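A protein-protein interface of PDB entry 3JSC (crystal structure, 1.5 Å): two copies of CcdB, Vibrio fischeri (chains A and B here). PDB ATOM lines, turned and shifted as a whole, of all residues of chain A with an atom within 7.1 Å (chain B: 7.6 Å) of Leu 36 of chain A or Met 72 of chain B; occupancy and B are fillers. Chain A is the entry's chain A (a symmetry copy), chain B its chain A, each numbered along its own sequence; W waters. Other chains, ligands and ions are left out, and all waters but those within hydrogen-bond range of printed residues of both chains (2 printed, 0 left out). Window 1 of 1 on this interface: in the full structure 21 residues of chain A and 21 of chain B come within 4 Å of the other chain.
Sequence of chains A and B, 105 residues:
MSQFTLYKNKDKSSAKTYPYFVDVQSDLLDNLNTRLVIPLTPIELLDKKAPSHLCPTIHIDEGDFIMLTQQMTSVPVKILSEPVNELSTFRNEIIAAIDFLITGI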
ATOM      1  N   PHE A  21      18.793 -17.060  34.756  1.00  0.00           N
ATOM      2  CA  PHE A  21      19.231 -17.644  33.508  1.00  0.00           C
ATOM      3  C   PHE A  21      19.049 -16.633  32.401  1.00  0.00           C
ATOM      4  O   PHE A  21      18.051 -15.896  32.397  1.00  0.00           O
ATOM      5  CB  PHE A  21      18.332 -18.843  33.119  1.00  0.00           C
ATOM      6  CG  PHE A  21      18.372 -20.006  34.084  1.00  0.00           C
ATOM      7  CD1 PHE A  21      17.212 -20.454  34.692  1.00  0.00           C
ATOM      8  CD2 PHE A  21      19.555 -20.664  34.340  1.00  0.00           C
ATOM      9  CE1 PHE A  21      17.244 -21.541  35.569  1.00  0.00           C
ATOM     10  CE2 PHE A  21      19.590 -21.769  35.231  1.00  0.00           C
ATOM     11  CZ  PHE A  21      18.417 -22.190  35.828  1.00  0.00           C
ATOM     12  N   VAL A  22      19.984 -16.582  31.456  1.00  0.00           N
ATOM     13  CA  VAL A  22      19.786 -15.874  30.191  1.00  0.00           C
ATOM     14  C   VAL A  22      19.369 -16.891  29.128  1.00  0.00           C
ATOM     15  O   VAL A  22      20.128 -17.820  28.844  1.00  0.00           O
ATOM     16  CB  VAL A  22      21.082 -15.199  29.735  1.00  0.00           C
ATOM     17  CG1 VAL A  22      20.846 -14.376  28.471  1.00  0.00           C
ATOM     18  CG2 VAL A  22      21.635 -14.323  30.846  1.00  0.00           C
ATOM     19  N   ASP A  23      18.182 -16.745  28.555  1.00  0.00           N
ATOM     20  CA  ASP A  23      17.694 -17.650  27.514  1.00  0.00           C
ATOM     21  C   ASP A  23      18.464 -17.343  26.218  1.00  0.00           C
ATOM     22  O   ASP A  23      18.568 -16.177  25.805  1.00  0.00           O
ATOM     23  CB  ASP A  23      16.197 -17.355  27.381  1.00  0.00           C
ATOM     24  CG  ASP A  23      15.489 -18.163  26.333  1.00  0.00           C
ATOM     25  OD1 ASP A  23      16.106 -18.780  25.444  1.00  0.00           O
ATOM     26  OD2 ASP A  23      14.232 -18.151  26.417  1.00  0.00           O
ATOM     27  N   VAL A  24      19.093 -18.362  25.630  1.00  0.00           N
ATOM     28  CA  VAL A  24      19.860 -18.167  24.383  1.00  0.00           C
ATOM     29  C   VAL A  24      19.339 -18.986  23.199  1.00  0.00           C
ATOM     30  O   VAL A  24      19.992 -19.058  22.164  1.00  0.00           O
ATOM     31  CB  VAL A  24      21.382 -18.404  24.596  1.00  0.00           C
ATOM     32  CG1 VAL A  24      21.926 -17.447  25.639  1.00  0.00           C
ATOM     33  CG2 VAL A  24      21.645 -19.836  25.047  1.00  0.00           C
ATOM     34  N   GLN A  25      18.138 -19.540  23.348  1.00  0.00           N
ATOM     35  CA  GLN A  25      17.545 -20.372  22.315  1.00  0.00           C
ATOM     36  C   GLN A  25      16.867 -19.557  21.233  1.00  0.00           C
ATOM     37  O   GLN A  25      16.293 -18.490  21.501  1.00  0.00           O
ATOM     38  CB  GLN A  25      16.522 -21.278  22.964  1.00  0.00           C
ATOM     39  CG  GLN A  25      15.965 -22.383  22.048  1.00  0.00           C
ATOM     40  CD  GLN A  25      15.437 -23.524  22.898  1.00  0.00           C
ATOM     41  OE1 GLN A  25      16.210 -24.224  23.540  1.00  0.00           O
ATOM     42  NE2 GLN A  25      14.109 -23.728  22.897  1.00  0.00           N
ATOM     43  N   SER A  26      16.884 -20.067  19.999  1.00  0.00           N
ATOM     44  CA  SER A  26      16.111 -19.426  18.935  1.00  0.00           C
ATOM     45  C   SER A  26      14.629 -19.336  19.290  1.00  0.00           C
ATOM     46  O   SER A  26      14.038 -20.316  19.727  1.00  0.00           O
ATOM     47  CB  SER A  26      16.237 -20.226  17.630  1.00  0.00           C
ATOM     48  OG  SER A  26      15.335 -19.672  16.659  1.00  0.00           O
ATOM     49  N   ASP A  30      10.768 -22.113  20.555  1.00  0.00           N
ATOM     50  CA  ASP A  30      10.381 -21.988  21.955  1.00  0.00           C
ATOM     51  C   ASP A  30       9.054 -22.665  22.338  1.00  0.00           C
ATOM     52  O   ASP A  30       8.613 -22.562  23.480  1.00  0.00           O
ATOM     53  CB  ASP A  30      10.468 -20.538  22.419  1.00  0.00           C
ATOM     54  CG  ASP A  30      11.898 -20.093  22.654  1.00  0.00           C
ATOM     55  OD1 ASP A  30      12.828 -20.930  22.589  1.00  0.00           O
ATOM     56  OD2 ASP A  30      12.090 -18.898  22.904  1.00  0.00           O
ATOM     57  N   THR A  34      11.924 -27.565  26.623  1.00  0.00           N
ATOM     58  CA  THR A  34      13.205 -27.193  27.245  1.00  0.00           C
ATOM     59  C   THR A  34      13.727 -25.903  26.619  1.00  0.00           C
ATOM     60  O   THR A  34      13.312 -25.498  25.535  1.00  0.00           O
ATOM     61  CB  THR A  34      14.266 -28.263  27.044  1.00  0.00           C
ATOM     62  OG1 THR A  34      14.353 -28.557  25.653  1.00  0.00           O
ATOM     63  CG2 THR A  34      13.914 -29.529  27.836  1.00  0.00           C
ATOM     64  N   ARG A  35      14.639 -25.250  27.323  1.00  0.00           N
ATOM     65  CA  ARG A  35      15.194 -23.993  26.842  1.00  0.00           C
ATOM     66  C   ARG A  35      16.684 -23.980  27.113  1.00  0.00           C
ATOM     67  O   ARG A  35      17.116 -24.199  28.246  1.00  0.00           O
ATOM     68  CB  ARG A  35      14.554 -22.860  27.632  1.00  0.00           C
ATOM     69  CG  ARG A  35      14.747 -21.489  27.025  1.00  0.00           C
ATOM     70  CD  ARG A  35      13.969 -21.283  25.687  1.00  0.00           C
ATOM     71  NE  ARG A  35      12.542 -21.622  25.716  1.00  0.00           N
ATOM     72  CZ  ARG A  35      11.589 -20.839  26.195  1.00  0.00           C
ATOM     73  NH1 ARG A  35      10.308 -21.231  26.183  1.00  0.00           N
ATOM     74  NH2 ARG A  35      11.924 -19.687  26.767  1.00  0.00           N
ATOM     75  N   LEU A  36      17.475 -23.715  26.075  1.00  0.00           N
ATOM     76  CA  LEU A  36      18.927 -23.539  26.245  1.00  0.00           C
ATOM     77  C   LEU A  36      19.181 -22.200  26.950  1.00  0.00           C
ATOM     78  O   LEU A  36      18.719 -21.140  26.483  1.00  0.00           O
ATOM     79  CB  LEU A  36      19.610 -23.545  24.863  1.00  0.00           C
ATOM     80  CG  LEU A  36      21.139 -23.549  24.904  1.00  0.00           C
ATOM     81  CD1 LEU A  36      21.670 -24.923  25.396  1.00  0.00           C
ATOM     82  CD2 LEU A  36      21.711 -23.270  23.512  1.00  0.00           C
ATOM     83  N   VAL A  37      19.917 -22.250  28.054  1.00  0.00           N
ATOM     84  CA  VAL A  37      20.148 -21.052  28.873  1.00  0.00           C
ATOM     85  C   VAL A  37      21.602 -20.987  29.327  1.00  0.00           C
ATOM     86  O   VAL A  37      22.305 -21.998  29.377  1.00  0.00           O
ATOM     87  CB  VAL A  37      19.266 -21.007  30.146  1.00  0.00           C
ATOM     88  CG1 VAL A  37      17.750 -20.980  29.792  1.00  0.00           C
ATOM     89  CG2 VAL A  37      19.602 -22.175  31.074  1.00  0.00           C
ATOM     90  N   ILE A  38      22.079 -19.782  29.628  1.00  0.00           N
ATOM     91  CA  ILE A  38      23.363 -19.617  30.327  1.00  0.00           C
ATOM     92  C   ILE A  38      23.051 -19.148  31.747  1.00  0.00           C
ATOM     93  O   ILE A  38      22.356 -18.144  31.940  1.00  0.00           O
ATOM     94  CB  ILE A  38      24.248 -18.578  29.620  1.00  0.00           C
ATOM     95  CG1 ILE A  38      24.620 -19.054  28.209  1.00  0.00           C
ATOM     96  CG2 ILE A  38      25.501 -18.323  30.467  1.00  0.00           C
ATOM     97  CD1 ILE A  38      25.364 -17.993  27.413  1.00  0.00           C
ATOM     98  N   MET A  72      26.550 -23.521  30.242  1.00  0.00           N
ATOM     99  CA  MET A  72      25.361 -23.469  29.387  1.00  0.00           C
ATOM    100  C   MET A  72      24.640 -24.808  29.442  1.00  0.00           C
ATOM    101  O   MET A  72      25.289 -25.860  29.418  1.00  0.00           O
ATOM    102  CB  MET A  72      25.741 -23.105  27.935  1.00  0.00           C
ATOM    103  CG  MET A  72      24.556 -22.983  26.998  1.00  0.00           C
ATOM    104  SD  MET A  72      25.010 -22.174  25.435  1.00  0.00           S
ATOM    105  CE  MET A  72      26.244 -23.336  24.863  1.00  0.00           C
ATOM    106  N   THR A  73      23.311 -24.789  29.509  1.00  0.00           N
ATOM    107  CA  THR A  73      22.557 -26.016  29.658  1.00  0.00           C
ATOM    108  C   THR A  73      21.128 -25.838  29.204  1.00  0.00           C
ATOM    109  O   THR A  73      20.645 -24.735  29.087  1.00  0.00           O
ATOM    110  CB  THR A  73      22.597 -26.495  31.129  1.00  0.00           C
ATOM    111  OG1 THR A  73      21.977 -27.784  31.227  1.00  0.00           O
ATOM    112  CG2 THR A  73      21.908 -25.497  32.068  1.00  0.00           C
ATOM    113  N   SER A  74      20.447 -26.941  28.973  1.00  0.00           N
ATOM    114  CA  SER A  74      19.037 -26.949  28.672  1.00  0.00           C
ATOM    115  C   SER A  74      18.286 -27.138  29.978  1.00  0.00           C
ATOM    116  O   SER A  74      18.701 -27.940  30.822  1.00  0.00           O
ATOM    117  CB  SER A  74      18.797 -28.120  27.723  1.00  0.00           C
ATOM    118  OG  SER A  74      17.443 -28.328  27.462  1.00  0.00           O
ATOM    119  N   VAL A  75      17.225 -26.369  30.193  1.00  0.00           N
ATOM    120  CA  VAL A  75      16.407 -26.526  31.389  1.00  0.00           C
ATOM    121  C   VAL A  75      14.942 -26.664  31.010  1.00  0.00           C
ATOM    122  O   VAL A  75      14.531 -26.229  29.955  1.00  0.00           O
ATOM    123  CB  VAL A  75      16.583 -25.359  32.402  1.00  0.00           C
ATOM    124  CG1 VAL A  75      18.031 -25.223  32.855  1.00  0.00           C
ATOM    125  CG2 VAL A  75      16.057 -24.016  31.865  1.00  0.00           C
ATOM    126  N   ILE A  98      29.591 -17.849  23.330  1.00  0.00           N
ATOM    127  CA  ILE A  98      29.196 -19.174  22.870  1.00  0.00           C
ATOM    128  C   ILE A  98      30.100 -19.645  21.731  1.00  0.00           C
ATOM    129  O   ILE A  98      30.557 -20.791  21.727  1.00  0.00           O
ATOM    130  CB  ILE A  98      27.723 -19.188  22.446  1.00  0.00           C
ATOM    131  CG1 ILE A  98      26.822 -18.978  23.672  1.00  0.00           C
ATOM    132  CG2 ILE A  98      27.390 -20.516  21.781  1.00  0.00           C
ATOM    133  CD1 ILE A  98      25.337 -18.728  23.304  1.00  0.00           C
ATOM    134  N   ILE A 102      32.743 -23.034  21.703  1.00  0.00           N
ATOM    135  CA  ILE A 102      32.671 -24.083  20.704  1.00  0.00           C
ATOM    136  C   ILE A 102      33.837 -24.055  19.719  1.00  0.00           C
ATOM    137  O   ILE A 102      34.342 -25.110  19.341  1.00  0.00           O
ATOM    138  CB  ILE A 102      31.301 -24.086  20.028  1.00  0.00           C
ATOM    139  CG1 ILE A 102      30.227 -24.401  21.068  1.00  0.00           C
ATOM    140  CG2 ILE A 102      31.271 -25.077  18.870  1.00  0.00           C
ATOM    141  CD1 ILE A 102      28.812 -24.092  20.594  1.00  0.00           C
ATOM    142  N   VAL B  22      28.228 -36.735  23.030  1.00  0.00           N
ATOM    143  CA  VAL B  22      29.162 -36.199  22.040  1.00  0.00           C
ATOM    144  C   VAL B  22      29.748 -34.895  22.585  1.00  0.00           C
ATOM    145  O   VAL B  22      28.999 -33.952  22.841  1.00  0.00           O
ATOM    146  CB  VAL B  22      28.445 -35.895  20.722  1.00  0.00           C
ATOM    147  CG1 VAL B  22      29.441 -35.435  19.660  1.00  0.00           C
ATOM    148  CG2 VAL B  22      27.685 -37.121  20.245  1.00  0.00           C
ATOM    149  N   VAL B  24      31.226 -31.395  22.402  1.00  0.00           N
ATOM    150  CA  VAL B  24      31.202 -30.334  21.374  1.00  0.00           C
ATOM    151  C   VAL B  24      31.983 -29.076  21.761  1.00  0.00           C
ATOM    152  O   VAL B  24      31.890 -28.059  21.083  1.00  0.00           O
ATOM    153  CB  VAL B  24      29.751 -29.977  20.944  1.00  0.00           C
ATOM    154  CG1 VAL B  24      29.051 -31.199  20.379  1.00  0.00           C
ATOM    155  CG2 VAL B  24      28.953 -29.448  22.130  1.00  0.00           C
ATOM    156  N   LEU B  36      31.027 -29.112  27.522  1.00  0.00           N
ATOM    157  CA  LEU B  36      29.761 -28.974  26.784  1.00  0.00           C
ATOM    158  C   LEU B  36      29.560 -30.222  25.914  1.00  0.00           C
ATOM    159  O   LEU B  36      30.439 -30.576  25.104  1.00  0.00           O
ATOM    160  CB  LEU B  36      29.819 -27.715  25.896  1.00  0.00           C
ATOM    161  CG  LEU B  36      28.501 -27.355  25.209  1.00  0.00           C
ATOM    162  CD1 LEU B  36      27.471 -26.822  26.243  1.00  0.00           C
ATOM    163  CD2 LEU B  36      28.731 -26.279  24.144  1.00  0.00           C
ATOM    164  N   VAL B  37      28.412 -30.869  26.073  1.00  0.00           N
ATOM    165  CA  VAL B  37      28.142 -32.131  25.372  1.00  0.00           C
ATOM    166  C   VAL B  37      26.714 -32.153  24.837  1.00  0.00           C
ATOM    167  O   VAL B  37      25.837 -31.437  25.323  1.00  0.00           O
ATOM    168  CB  VAL B  37      28.313 -33.378  26.276  1.00  0.00           C
ATOM    169  CG1 VAL B  37      29.771 -33.504  26.808  1.00  0.00           C
ATOM    170  CG2 VAL B  37      27.300 -33.353  27.421  1.00  0.00           C
ATOM    171  N   ILE B  38      26.478 -32.950  23.800  1.00  0.00           N
ATOM    172  CA  ILE B  38      25.107 -33.264  23.368  1.00  0.00           C
ATOM    173  C   ILE B  38      24.835 -34.720  23.739  1.00  0.00           C
ATOM    174  O   ILE B  38      25.591 -35.620  23.356  1.00  0.00           O
ATOM    175  CB  ILE B  38      24.948 -33.076  21.852  1.00  0.00           C
ATOM    176  CG1 ILE B  38      25.165 -31.607  21.462  1.00  0.00           C
ATOM    177  CG2 ILE B  38      23.558 -33.564  21.425  1.00  0.00           C
ATOM    178  CD1 ILE B  38      25.172 -31.398  19.956  1.00  0.00           C
ATOM    179  N   PRO B  39      23.790 -34.982  24.527  1.00  0.00           N
ATOM    180  CA  PRO B  39      23.447 -36.376  24.860  1.00  0.00           C
ATOM    181  C   PRO B  39      22.835 -37.160  23.695  1.00  0.00           C
ATOM    182  O   PRO B  39      22.146 -36.573  22.849  1.00  0.00           O
ATOM    183  CB  PRO B  39      22.403 -36.254  25.978  1.00  0.00           C
ATOM    184  CG  PRO B  39      22.177 -34.798  26.180  1.00  0.00           C
ATOM    185  CD  PRO B  39      22.869 -34.003  25.122  1.00  0.00           C
ATOM    186  N   LEU B  68      20.410 -35.453  20.771  1.00  0.00           N
ATOM    187  CA  LEU B  68      19.465 -34.543  21.421  1.00  0.00           C
ATOM    188  C   LEU B  68      20.041 -33.162  21.621  1.00  0.00           C
ATOM    189  O   LEU B  68      20.312 -32.726  22.747  1.00  0.00           O
ATOM    190  CB  LEU B  68      18.985 -35.116  22.751  1.00  0.00           C
ATOM    191  CG  LEU B  68      18.177 -36.406  22.702  1.00  0.00           C
ATOM    192  CD1 LEU B  68      18.023 -36.914  24.127  1.00  0.00           C
ATOM    193  CD2 LEU B  68      16.829 -36.161  22.065  1.00  0.00           C
ATOM    194  N   THR B  69      20.199 -32.473  20.506  1.00  0.00           N
ATOM    195  CA  THR B  69      20.778 -31.141  20.509  1.00  0.00           C
ATOM    196  C   THR B  69      20.034 -30.202  21.453  1.00  0.00           C
ATOM    197  O   THR B  69      20.668 -29.347  22.099  1.00  0.00           O
ATOM    198  CB  THR B  69      20.787 -30.549  19.107  1.00  0.00           C
ATOM    199  OG1 THR B  69      21.295 -31.532  18.197  1.00  0.00           O
ATOM    200  CG2 THR B  69      21.686 -29.315  19.056  1.00  0.00           C
ATOM    201  N   GLN B  70      18.717 -30.344  21.552  1.00  0.00           N
ATOM    202  CA  GLN B  70      18.007 -29.397  22.404  1.00  0.00           C
ATOM    203  C   GLN B  70      18.297 -29.627  23.882  1.00  0.00           C
ATOM    204  O   GLN B  70      17.994 -28.757  24.713  1.00  0.00           O
ATOM    205  CB  GLN B  70      16.515 -29.366  22.110  1.00  0.00           C
ATOM    206  CG  GLN B  70      15.737 -30.476  22.731  1.00  0.00           C
ATOM    207  CD  GLN B  70      15.777 -31.749  21.933  1.00  0.00           C
ATOM    208  NE2 GLN B  70      14.777 -32.600  22.151  1.00  0.00           N
ATOM    209  N   GLN B  71      18.895 -30.781  24.207  1.00  0.00           N
ATOM    210  CA  GLN B  71      19.289 -31.073  25.580  1.00  0.00           C
ATOM    211  C   GLN B  71      20.801 -30.930  25.793  1.00  0.00           C
ATOM    212  O   GLN B  71      21.364 -31.490  26.750  1.00  0.00           O
ATOM    213  CB  GLN B  71      18.784 -32.451  25.991  1.00  0.00           C
ATOM    214  CG  GLN B  71      17.263 -32.578  25.834  1.00  0.00           C
ATOM    215  CD  GLN B  71      16.735 -33.862  26.420  1.00  0.00           C
ATOM    216  OE1 GLN B  71      17.212 -34.318  27.452  1.00  0.00           O
ATOM    217  NE2 GLN B  71      15.749 -34.457  25.763  1.00  0.00           N
ATOM    218  N   MET B  72      21.444 -30.164  24.910  1.00  0.00           N
ATOM    219  CA  MET B  72      22.862 -29.828  25.063  1.00  0.00           C
ATOM    220  C   MET B  72      23.107 -29.293  26.467  1.00  0.00           C
ATOM    221  O   MET B  72      22.299 -28.511  26.979  1.00  0.00           O
ATOM    222  CB  MET B  72      23.305 -28.803  23.996  1.00  0.00           C
ATOM    223  CG  MET B  72      24.776 -28.442  24.058  1.00  0.00           C
ATOM    224  SD  MET B  72      25.320 -27.564  22.563  1.00  0.00           S
ATOM    225  CE  MET B  72      24.241 -26.141  22.662  1.00  0.00           C
ATOM    226  N   THR B  73      24.209 -29.697  27.095  1.00  0.00           N
ATOM    227  CA  THR B  73      24.467 -29.308  28.466  1.00  0.00           C
ATOM    228  C   THR B  73      25.935 -29.419  28.799  1.00  0.00           C
ATOM    229  O   THR B  73      26.681 -30.078  28.111  1.00  0.00           O
ATOM    230  CB  THR B  73      23.629 -30.176  29.436  1.00  0.00           C
ATOM    231  OG1 THR B  73      23.782 -29.677  30.772  1.00  0.00           O
ATOM    232  CG2 THR B  73      24.035 -31.653  29.367  1.00  0.00           C
ATOM    233  N   SER B  74      26.339 -28.785  29.880  1.00  0.00           N
ATOM    234  CA  SER B  74      27.673 -28.905  30.413  1.00  0.00           C
ATOM    235  C   SER B  74      27.658 -30.010  31.453  1.00  0.00           C
ATOM    236  O   SER B  74      26.710 -30.108  32.241  1.00  0.00           O
ATOM    237  CB  SER B  74      28.017 -27.558  31.043  1.00  0.00           C
ATOM    238  OG  SER B  74      29.234 -27.581  31.723  1.00  0.00           O
ATOM    239  N   VAL B  75      28.655 -30.887  31.433  1.00  0.00           N
ATOM    240  CA  VAL B  75      28.756 -31.941  32.433  1.00  0.00           C
ATOM    241  C   VAL B  75      30.139 -31.940  33.062  1.00  0.00           C
ATOM    242  O   VAL B  75      31.088 -31.468  32.471  1.00  0.00           O
ATOM    243  CB  VAL B  75      28.436 -33.352  31.863  1.00  0.00           C
ATOM    244  CG1 VAL B  75      27.032 -33.414  31.275  1.00  0.00           C
ATOM    245  CG2 VAL B  75      29.474 -33.831  30.832  1.00  0.00           C
ATOM    246  N   ILE B  94      26.610 -31.627  13.264  1.00  0.00           N
ATOM    247  CA  ILE B  94      26.522 -31.216  14.669  1.00  0.00           C
ATOM    248  C   ILE B  94      26.515 -29.690  14.771  1.00  0.00           C
ATOM    249  O   ILE B  94      25.658 -29.094  15.454  1.00  0.00           O
ATOM    250  CB  ILE B  94      27.682 -31.840  15.469  1.00  0.00           C
ATOM    251  CG1 ILE B  94      27.442 -33.334  15.607  1.00  0.00           C
ATOM    252  CG2 ILE B  94      27.787 -31.199  16.886  1.00  0.00           C
ATOM    253  CD1 ILE B  94      28.663 -34.121  16.100  1.00  0.00           C
ATOM    254  N   ALA B  97      23.252 -28.292  13.607  1.00  0.00           N
ATOM    255  CA  ALA B  97      22.186 -28.489  14.581  1.00  0.00           C
ATOM    256  C   ALA B  97      22.290 -27.447  15.692  1.00  0.00           C
ATOM    257  O   ALA B  97      21.271 -26.861  16.096  1.00  0.00           O
ATOM    258  CB  ALA B  97      22.229 -29.914  15.154  1.00  0.00           C
ATOM    259  N   ILE B  98      23.510 -27.207  16.182  1.00  0.00           N
ATOM    260  CA  ILE B  98      23.719 -26.196  17.209  1.00  0.00           C
ATOM    261  C   ILE B  98      23.360 -24.806  16.684  1.00  0.00           C
ATOM    262  O   ILE B  98      22.681 -24.034  17.366  1.00  0.00           O
ATOM    263  CB  ILE B  98      25.163 -26.231  17.725  1.00  0.00           C
ATOM    264  CG1 ILE B  98      25.414 -27.540  18.490  1.00  0.00           C
ATOM    265  CG2 ILE B  98      25.415 -25.042  18.639  1.00  0.00           C
ATOM    266  CD1 ILE B  98      26.909 -27.773  18.827  1.00  0.00           C
ATOM    267  N   ASP B  99      23.766 -24.505  15.460  1.00  0.00           N
ATOM    268  CA  ASP B  99      23.433 -23.210  14.855  1.00  0.00           C
ATOM    269  C   ASP B  99      21.918 -23.066  14.722  1.00  0.00           C
ATOM    270  O   ASP B  99      21.382 -21.973  14.930  1.00  0.00           O
ATOM    271  CB  ASP B  99      24.101 -23.087  13.480  1.00  0.00           C
ATOM    272  CG  ASP B  99      25.593 -22.835  13.562  1.00  0.00           C
ATOM    273  OD1 ASP B  99      26.109 -22.532  14.654  1.00  0.00           O
ATOM    274  OD2 ASP B  99      26.273 -22.977  12.518  1.00  0.00           O
ATOM    275  N   LEU B 101      19.612 -24.495  16.666  1.00  0.00           N
ATOM    276  CA  LEU B 101      19.074 -24.313  18.015  1.00  0.00           C
ATOM    277  C   LEU B 101      19.173 -22.852  18.472  1.00  0.00           C
ATOM    278  O   LEU B 101      18.266 -22.351  19.146  1.00  0.00           O
ATOM    279  CB  LEU B 101      19.824 -25.221  18.970  1.00  0.00           C
ATOM    280  CG  LEU B 101      19.435 -25.121  20.441  1.00  0.00           C
ATOM    281  CD1 LEU B 101      17.999 -25.493  20.621  1.00  0.00           C
ATOM    282  CD2 LEU B 101      20.376 -26.058  21.207  1.00  0.00           C
ATOM    283  N   ILE B 102      20.263 -22.182  18.098  1.00  0.00           N
ATOM    284  CA  ILE B 102      20.519 -20.822  18.535  1.00  0.00           C
ATOM    285  C   ILE B 102      19.992 -19.771  17.562  1.00  0.00           C
ATOM    286  O   ILE B 102      19.469 -18.746  17.996  1.00  0.00           O
ATOM    287  CB  ILE B 102      21.994 -20.642  18.888  1.00  0.00           C
ATOM    288  CG1 ILE B 102      22.344 -21.551  20.066  1.00  0.00           C
ATOM    289  CG2 ILE B 102      22.303 -19.180  19.194  1.00  0.00           C
ATOM    290  CD1 ILE B 102      23.844 -21.717  20.282  1.00  0.00           C
HETATM  291  O   HOH W   1      13.864 -31.249  25.194  1.00  0.00           O
HETATM  292  O   HOH W   2      16.090 -26.821  24.561  1.00  0.00           O
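N of Ser 74 of chain B lies within hydrogen-bond range of O of Met 72 of chain A.
The backbone NH of Ser 26 of chain A lies within hydrogen-bond range of the backbone carbonyl oxygen of Leu 101 of chain B, at 2.8 Å.
The backbone NH (N) of Ser 74 of chain A is in hydrogen-bond range of the backbone carbonyl oxygen (O) of Met 72 of chain B (3.1 Å).
O of Gln 70 of chain B sits at hydrogen-bond distance from OG of Ser 74 of chain A (2.8 Å).
OG1 of Thr 73 of chain A is in hydrogen-bond range of OG1 of Thr 73 of chain B (2.7 Å).
The backbone NH (N) of Leu 36 of chain A sits at hydrogen-bond distance from the side-chain amide oxygen (OE1) of Gln 25 of chain A, 2.9 Å away.
OD1 of Asp 30 of chain A is in hydrogen-bond range of NE2 of Gln 25 of chain A.
The side-chain amide nitrogen (NE2) of Gln 25 of chain A is in hydrogen-bond range of the backbone carbonyl oxygen (O) of Thr 34 of chain A (3.3 Å).
N of Val 37 of chain B sits at hydrogen-bond distance from O of Thr 73 of chain B (2.8 Å).
The backbone NH (N) of Val 24 of chain A lies within hydrogen-bond range of the backbone carbonyl oxygen (O) of Leu 36 of chain A.
The side-chain carboxylate of Asp 23 of chain A is in hydrogen-bond range of the backbone NH of Gln 25 of chain A (3.0 Å).
OE1 of Gln 25 of chain A touches CD1 of Leu 101 of chain B, at 3.7 Å.
Thr 34 of chain A touches Gln 70 of chain B.
CD2 of Leu 36 of chain A touches CE of Met 72 of chain B (3.9 Å).
Leu 101 of chain B touches Leu 36 of chain A (CD2 to CD2, 3.9 Å).
Leu 36 of chain A touches Ile 102 of chain B.
Leu 36 of chain B touches Met 72 of chain A (CD2 to CE, 3.9 Å).
Thr 73 of chain B touches Met 72 of chain A.
C of Thr 73 of chain A touches O of Met 72 of chain B (3.7 Å).
Val 24 of chain B touches Ile 102 of chain A.
Ile 102 of chain A touches Leu 36 of chain B (CG1 to CD2, 3.9 Å).
Leu 36 of chain A touches just these residues of chain B: Met 72 (3.9 Å), Leu 101 (3.9 Å) and Ile 102 (3.9 Å).
Printed residues of chain A within 4 Å of Met 72 of chain B: Leu 36 (3.9 Å), Thr 73 (3.7 Å) and Ser 74 (3.1 Å).
Printed residues of chain A within 4 Å of Ile 102 of chain B: Val 24 (3.8 Å), Ser 26 (3.5 Å) and Leu 36 (3.9 Å).
Printed residues of chain A within 4 Å of Leu 36 of chain B: Met 72 and Ile 102.
Printed residues of chain A within 4 Å of Leu 101 of chain B: Gln 25 (3.7 Å), Ser 26 (2.8 Å) and Leu 36 (3.9 Å).
Printed residues of chain A within 4 Å of Val 24 of chain B: Ile 102.
The nearest residue of chain B that does not touch Leu 36 of chain A is Gln 70 of chain B (5.2 Å).
The nearest residue of chain A that does not touch Met 72 of chain B is Met 72 of chain A (4.1 Å).
The nearest printed residue of chain A that does not touch Val 24 of chain B is Met 72 of chain A (7.2 Å).
Along chain B the printed residues that touch a printed residue of chain A span positions 24 to 102.
Printed residues of chain A that touch a printed residue of chain B: Val 24, Gln 25, Ser 26, Thr 34, Leu 36, Met 72, Thr 73, Ser 74 and Ile 102.
Among the printed residues, 18 pairs touch across the chains.
Among the printed residues, no Asp or Glu carboxylate lies within 4 Å of a Lys or Arg side-chain nitrogen of the other chain.
Val 24 of chain A touches Ile 102 of chain B, and with the chains exchanged Ile 102 of chain A touches Val 24 of chain B.
Leu 36 of chain A touches Met 72 of chain B, and with the chains exchanged Met 72 of chain A touches Leu 36 of chain B.
Leu 36 of chain A touches Ile 102 of chain B, and with the chains exchanged Ile 102 of chain A touches Leu 36 of chain B.
Thr 73 of chain A touches its own counterpart, Thr 73 of chain B.
11 positions are printed for both chains.
Of the 18 pairs that touch across the chains among the printed residues, 11 have their exchanged pair printed and touching as well.
Water W2 lies within hydrogen-bond range of OG1 of Thr 34 of chain A (2.7 Å), O of Gln 70 of chain B (2.7 Å), OE1 of Gln 25 of chain A (2.8 Å) and N of Arg 35 of chain A (3.5 Å).
Water W1 bridges OG1 of Thr 34 of chain A (2.8 Å) and NE2 of Gln 70 of chain B (3.5 Å).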
